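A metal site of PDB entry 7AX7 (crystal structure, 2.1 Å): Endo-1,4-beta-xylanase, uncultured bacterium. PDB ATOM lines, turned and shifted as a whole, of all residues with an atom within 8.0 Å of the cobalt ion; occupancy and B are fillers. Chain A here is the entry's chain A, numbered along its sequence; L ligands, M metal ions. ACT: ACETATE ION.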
ATOM      1  N   PHE A  10      14.041  20.986 -15.796  1.00  0.00           N
ATOM      2  CA  PHE A  10      12.657  21.423 -15.805  1.00  0.00           C
ATOM      3  C   PHE A  10      11.760  20.339 -15.233  1.00  0.00           C
ATOM      4  O   PHE A  10      11.812  19.184 -15.666  1.00  0.00           O
ATOM      5  CB  PHE A  10      12.216  21.774 -17.237  1.00  0.00           C
ATOM      6  CG  PHE A  10      12.923  22.962 -17.825  1.00  0.00           C
ATOM      7  CD1 PHE A  10      12.427  24.243 -17.646  1.00  0.00           C
ATOM      8  CD2 PHE A  10      14.097  22.789 -18.567  1.00  0.00           C
ATOM      9  CE1 PHE A  10      13.063  25.344 -18.195  1.00  0.00           C
ATOM     10  CE2 PHE A  10      14.750  23.885 -19.116  1.00  0.00           C
ATOM     11  CZ  PHE A  10      14.237  25.171 -18.937  1.00  0.00           C
ATOM     12  N   ASP A  11      10.934  20.728 -14.255  1.00  0.00           N
ATOM     13  CA  ASP A  11       9.969  19.849 -13.581  1.00  0.00           C
ATOM     14  C   ASP A  11       8.542  20.086 -14.081  1.00  0.00           C
ATOM     15  O   ASP A  11       8.157  21.221 -14.370  1.00  0.00           O
ATOM     16  CB  ASP A  11       9.975  20.091 -12.068  1.00  0.00           C
ATOM     17  CG  ASP A  11      11.093  19.382 -11.349  1.00  0.00           C
ATOM     18  OD1 ASP A  11      11.882  18.656 -12.011  1.00  0.00           O
ATOM     19  OD2 ASP A  11      11.159  19.533 -10.110  1.00  0.00           O
ATOM     20  N   ASP A  12       7.765  18.999 -14.133  1.00  0.00           N
ATOM     21  CA  ASP A  12       6.299  18.985 -14.121  1.00  0.00           C
ATOM     22  C   ASP A  12       5.672  18.838 -15.507  1.00  0.00           C
ATOM     23  O   ASP A  12       4.439  18.790 -15.612  1.00  0.00           O
ATOM     24  CB  ASP A  12       5.748  20.250 -13.441  1.00  0.00           C
ATOM     25  CG  ASP A  12       6.045  20.302 -11.945  1.00  0.00           C
ATOM     26  OD1 ASP A  12       6.681  19.360 -11.392  1.00  0.00           O
ATOM     27  OD2 ASP A  12       5.640  21.282 -11.300  1.00  0.00           O
ATOM     28  N   GLY A  13       6.463  18.745 -16.569  1.00  0.00           N
ATOM     29  CA  GLY A  13       5.908  18.518 -17.896  1.00  0.00           C
ATOM     30  C   GLY A  13       5.695  17.045 -18.216  1.00  0.00           C
ATOM     31  O   GLY A  13       5.704  16.186 -17.332  1.00  0.00           O
ATOM     32  N   PHE A  35      12.346  16.432 -16.003  1.00  0.00           N
ATOM     33  CA  PHE A  35      11.812  15.454 -15.059  1.00  0.00           C
ATOM     34  C   PHE A  35      10.301  15.408 -15.233  1.00  0.00           C
ATOM     35  O   PHE A  35       9.595  16.349 -14.858  1.00  0.00           O
ATOM     36  CB  PHE A  35      12.234  15.826 -13.633  1.00  0.00           C
ATOM     37  CG  PHE A  35      13.708  15.665 -13.369  1.00  0.00           C
ATOM     38  CD1 PHE A  35      14.609  16.613 -13.814  1.00  0.00           C
ATOM     39  CD2 PHE A  35      14.186  14.550 -12.683  1.00  0.00           C
ATOM     40  CE1 PHE A  35      15.985  16.467 -13.578  1.00  0.00           C
ATOM     41  CE2 PHE A  35      15.553  14.389 -12.448  1.00  0.00           C
ATOM     42  CZ  PHE A  35      16.456  15.349 -12.899  1.00  0.00           C
ATOM     43  N   ILE A  37       6.323  14.127 -15.142  1.00  0.00           N
ATOM     44  CA  ILE A  37       5.257  13.495 -14.377  1.00  0.00           C
ATOM     45  C   ILE A  37       4.655  12.395 -15.251  1.00  0.00           C
ATOM     46  O   ILE A  37       4.206  12.661 -16.369  1.00  0.00           O
ATOM     47  CB  ILE A  37       4.200  14.532 -13.968  1.00  0.00           C
ATOM     48  CG1 ILE A  37       4.855  15.600 -13.089  1.00  0.00           C
ATOM     49  CG2 ILE A  37       3.021  13.843 -13.262  1.00  0.00           C
ATOM     50  CD1 ILE A  37       3.938  16.742 -12.689  1.00  0.00           C
ATOM     51  N   HIS A  62       9.787  12.295 -12.491  1.00  0.00           N
ATOM     52  CA  HIS A  62       9.251  13.133 -11.428  1.00  0.00           C
ATOM     53  C   HIS A  62       8.058  12.459 -10.728  1.00  0.00           C
ATOM     54  O   HIS A  62       7.176  13.141 -10.203  1.00  0.00           O
ATOM     55  CB  HIS A  62       8.876  14.504 -11.988  1.00  0.00           C
ATOM     56  CG  HIS A  62       8.820  15.607 -10.978  1.00  0.00           C
ATOM     57  ND1 HIS A  62       9.592  15.609  -9.826  1.00  0.00           N
ATOM     58  CD2 HIS A  62       8.119  16.763 -10.946  1.00  0.00           C
ATOM     59  CE1 HIS A  62       9.353  16.703  -9.133  1.00  0.00           C
ATOM     60  NE2 HIS A  62       8.457  17.429  -9.795  1.00  0.00           N
ATOM     61  N   SER A  63       8.039  11.131 -10.731  1.00  0.00           N
ATOM     62  CA  SER A  63       6.948  10.283 -10.217  1.00  0.00           C
ATOM     63  C   SER A  63       5.792  10.183 -11.224  1.00  0.00           C
ATOM     64  O   SER A  63       5.847  10.796 -12.291  1.00  0.00           O
ATOM     65  CB  SER A  63       6.429  10.785  -8.859  1.00  0.00           C
ATOM     66  OG  SER A  63       5.434  11.791  -9.011  1.00  0.00           O
ATOM     67  N   HIS A  66       2.686  12.783  -9.031  1.00  0.00           N
ATOM     68  CA  HIS A  66       3.185  14.028  -8.446  1.00  0.00           C
ATOM     69  C   HIS A  66       2.502  14.340  -7.112  1.00  0.00           C
ATOM     70  O   HIS A  66       2.018  15.449  -6.871  1.00  0.00           O
ATOM     71  CB  HIS A  66       3.028  15.199  -9.428  1.00  0.00           C
ATOM     72  CG  HIS A  66       3.886  16.373  -9.104  1.00  0.00           C
ATOM     73  ND1 HIS A  66       3.449  17.420  -8.314  1.00  0.00           N
ATOM     74  CD2 HIS A  66       5.169  16.661  -9.419  1.00  0.00           C
ATOM     75  CE1 HIS A  66       4.428  18.306  -8.181  1.00  0.00           C
ATOM     76  NE2 HIS A  66       5.477  17.867  -8.843  1.00  0.00           N
ATOM     77  N   ARG A 100      13.642  13.071  -9.498  1.00  0.00           N
ATOM     78  CA  ARG A 100      13.541  14.249  -8.639  1.00  0.00           C
ATOM     79  C   ARG A 100      12.250  14.171  -7.832  1.00  0.00           C
ATOM     80  O   ARG A 100      11.168  14.061  -8.429  1.00  0.00           O
ATOM     81  CB  ARG A 100      13.599  15.537  -9.439  1.00  0.00           C
ATOM     82  CG  ARG A 100      13.470  16.779  -8.577  1.00  0.00           C
ATOM     83  CD  ARG A 100      13.535  18.020  -9.464  1.00  0.00           C
ATOM     84  NE  ARG A 100      14.902  18.500  -9.614  1.00  0.00           N
ATOM     85  CZ  ARG A 100      15.362  19.105 -10.711  1.00  0.00           C
ATOM     86  NH1 ARG A 100      14.584  19.291 -11.769  1.00  0.00           N
ATOM     87  NH2 ARG A 100      16.610  19.516 -10.745  1.00  0.00           N
ATOM     88  N   PRO A 101      12.328  14.203  -6.507  1.00  0.00           N
ATOM     89  CA  PRO A 101      11.125  14.010  -5.684  1.00  0.00           C
ATOM     90  C   PRO A 101      10.172  15.185  -5.792  1.00  0.00           C
ATOM     91  O   PRO A 101      10.589  16.355  -5.721  1.00  0.00           O
ATOM     92  CB  PRO A 101      11.688  13.876  -4.269  1.00  0.00           C
ATOM     93  CG  PRO A 101      13.009  14.549  -4.304  1.00  0.00           C
ATOM     94  CD  PRO A 101      13.548  14.286  -5.692  1.00  0.00           C
ATOM     95  N   PRO A 102       8.870  14.924  -5.957  1.00  0.00           N
ATOM     96  CA  PRO A 102       7.889  16.015  -5.956  1.00  0.00           C
ATOM     97  C   PRO A 102       7.981  16.818  -4.656  1.00  0.00           C
ATOM     98  O   PRO A 102       8.083  16.250  -3.566  1.00  0.00           O
ATOM     99  CB  PRO A 102       6.546  15.297  -6.065  1.00  0.00           C
ATOM    100  CG  PRO A 102       6.882  13.959  -6.720  1.00  0.00           C
ATOM    101  CD  PRO A 102       8.242  13.605  -6.176  1.00  0.00           C
ATOM    102  N   TYR A 103       7.943  18.140  -4.795  1.00  0.00           N
ATOM    103  CA  TYR A 103       8.049  19.077  -3.680  1.00  0.00           C
ATOM    104  C   TYR A 103       9.376  18.971  -2.939  1.00  0.00           C
ATOM    105  O   TYR A 103       9.526  19.559  -1.869  1.00  0.00           O
ATOM    106  CB  TYR A 103       6.878  18.912  -2.700  1.00  0.00           C
ATOM    107  CG  TYR A 103       5.560  18.837  -3.443  1.00  0.00           C
ATOM    108  CD1 TYR A 103       5.003  19.988  -4.000  1.00  0.00           C
ATOM    109  CD2 TYR A 103       4.914  17.630  -3.642  1.00  0.00           C
ATOM    110  CE1 TYR A 103       3.811  19.923  -4.707  1.00  0.00           C
ATOM    111  CE2 TYR A 103       3.723  17.564  -4.350  1.00  0.00           C
ATOM    112  CZ  TYR A 103       3.183  18.710  -4.879  1.00  0.00           C
ATOM    113  OH  TYR A 103       2.000  18.659  -5.585  1.00  0.00           O
ATOM    114  N   ILE A 104      10.342  18.240  -3.495  1.00  0.00           N
ATOM    115  CA  ILE A 104      11.570  17.917  -2.786  1.00  0.00           C
ATOM    116  C   ILE A 104      11.187  17.408  -1.401  1.00  0.00           C
ATOM    117  O   ILE A 104      11.818  17.760  -0.395  1.00  0.00           O
ATOM    118  CB  ILE A 104      12.516  19.130  -2.708  1.00  0.00           C
ATOM    119  CG1 ILE A 104      12.579  19.859  -4.045  1.00  0.00           C
ATOM    120  CG2 ILE A 104      13.910  18.687  -2.274  1.00  0.00           C
ATOM    121  CD1 ILE A 104      13.253  19.063  -5.163  1.00  0.00           C
ATOM    122  N   SER A 127       7.775  28.648  -9.447  1.00  0.00           N
ATOM    123  CA  SER A 127       6.473  28.004  -9.382  1.00  0.00           C
ATOM    124  C   SER A 127       5.351  28.961  -8.998  1.00  0.00           C
ATOM    125  O   SER A 127       4.178  28.636  -9.188  1.00  0.00           O
ATOM    126  CB  SER A 127       6.502  26.810  -8.401  1.00  0.00           C
ATOM    127  OG  SER A 127       6.526  27.231  -7.049  1.00  0.00           O
ATOM    128  N   LEU A 151      16.987  24.143 -10.969  1.00  0.00           N
ATOM    129  CA  LEU A 151      15.627  23.601 -11.041  1.00  0.00           C
ATOM    130  C   LEU A 151      14.673  24.705 -11.499  1.00  0.00           C
ATOM    131  O   LEU A 151      14.519  25.728 -10.818  1.00  0.00           O
ATOM    132  CB  LEU A 151      15.211  23.045  -9.679  1.00  0.00           C
ATOM    133  CG  LEU A 151      13.902  22.255  -9.587  1.00  0.00           C
ATOM    134  CD1 LEU A 151      13.910  21.366  -8.357  1.00  0.00           C
ATOM    135  CD2 LEU A 151      12.677  23.164  -9.580  1.00  0.00           C
ATOM    136  N   LEU A 152      14.050  24.484 -12.655  1.00  0.00           N
ATOM    137  CA  LEU A 152      12.973  25.321 -13.191  1.00  0.00           C
ATOM    138  C   LEU A 152      11.727  24.452 -13.378  1.00  0.00           C
ATOM    139  O   LEU A 152      11.770  23.238 -13.170  1.00  0.00           O
ATOM    140  CB  LEU A 152      13.419  25.985 -14.504  1.00  0.00           C
ATOM    141  CG  LEU A 152      14.700  26.833 -14.466  1.00  0.00           C
ATOM    142  CD1 LEU A 152      15.943  25.964 -14.669  1.00  0.00           C
ATOM    143  CD2 LEU A 152      14.672  27.922 -15.509  1.00  0.00           C
ATOM    144  N   HIS A 153      10.605  25.066 -13.769  1.00  0.00           N
ATOM    145  CA  HIS A 153       9.352  24.339 -13.999  1.00  0.00           C
ATOM    146  C   HIS A 153       8.798  24.628 -15.378  1.00  0.00           C
ATOM    147  O   HIS A 153       8.775  25.786 -15.823  1.00  0.00           O
ATOM    148  CB  HIS A 153       8.264  24.709 -12.972  1.00  0.00           C
ATOM    149  CG  HIS A 153       8.629  24.413 -11.558  1.00  0.00           C
ATOM    150  ND1 HIS A 153       9.560  25.152 -10.859  1.00  0.00           N
ATOM    151  CD2 HIS A 153       8.176  23.463 -10.697  1.00  0.00           C
ATOM    152  CE1 HIS A 153       9.655  24.683  -9.629  1.00  0.00           C
ATOM    153  NE2 HIS A 153       8.834  23.655  -9.508  1.00  0.00           N
ATOM    154  N   PHE A 155       5.492  23.339 -16.061  1.00  0.00           N
ATOM    155  CA  PHE A 155       4.070  23.025 -16.001  1.00  0.00           C
ATOM    156  C   PHE A 155       3.296  23.981 -16.921  1.00  0.00           C
ATOM    157  O   PHE A 155       3.783  25.061 -17.287  1.00  0.00           O
ATOM    158  CB  PHE A 155       3.534  23.101 -14.566  1.00  0.00           C
ATOM    159  CG  PHE A 155       3.729  24.438 -13.891  1.00  0.00           C
ATOM    160  CD1 PHE A 155       2.904  25.504 -14.203  1.00  0.00           C
ATOM    161  CD2 PHE A 155       4.709  24.607 -12.944  1.00  0.00           C
ATOM    162  CE1 PHE A 155       3.079  26.748 -13.575  1.00  0.00           C
ATOM    163  CE2 PHE A 155       4.892  25.833 -12.317  1.00  0.00           C
ATOM    164  CZ  PHE A 155       4.063  26.908 -12.629  1.00  0.00           C
HETATM  165  C   ACT L   1       8.883  20.081  -7.703  1.00  0.00           C
HETATM  166  O   ACT L   1       9.003  20.371  -8.928  1.00  0.00           O
HETATM  167  OXT ACT L   1       7.958  19.433  -7.131  1.00  0.00           O
HETATM  168  CH3 ACT L   1      10.047  20.594  -6.790  1.00  0.00           C
HETATM  169 CO    CO M   1       7.129  19.163  -9.308  1.00  0.00          CO
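Within 4 Å of the cobalt ion: Asp 12, His 62 and His 66.
A ring nitrogen (ND1) of His 66 is in hydrogen-bond range of the side-chain hydroxyl (OH) of Tyr 103, 3.3 Å away.
N of His 66 sits at hydrogen-bond distance from OG of Ser 63 (2.9 Å).
A ring nitrogen (NE2) of His 62 lies close to the side-chain carboxylate (OD2) of Asp 11, at 3.4 Å.
The backbone NH (N) of Asp 12 sits at hydrogen-bond distance from the backbone carbonyl oxygen (O) of Phe 35.
A ring nitrogen (ND1) of His 62 lies within hydrogen-bond range of the backbone carbonyl oxygen of Arg 100 (2.6 Å).
The cobalt ion is bound by the side-chain carboxylate of Asp 12 (2.1 Å), a ring nitrogen (NE2) of His 66 (2.2 Å), a ring nitrogen (NE2) of His 62 (2.2 Å), an oxygen (O) of the ligand (2.3 Å) and an oxygen (OXT) of the ligand (2.3 Å).
The cobalt ion has five donor atoms within binding distance.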
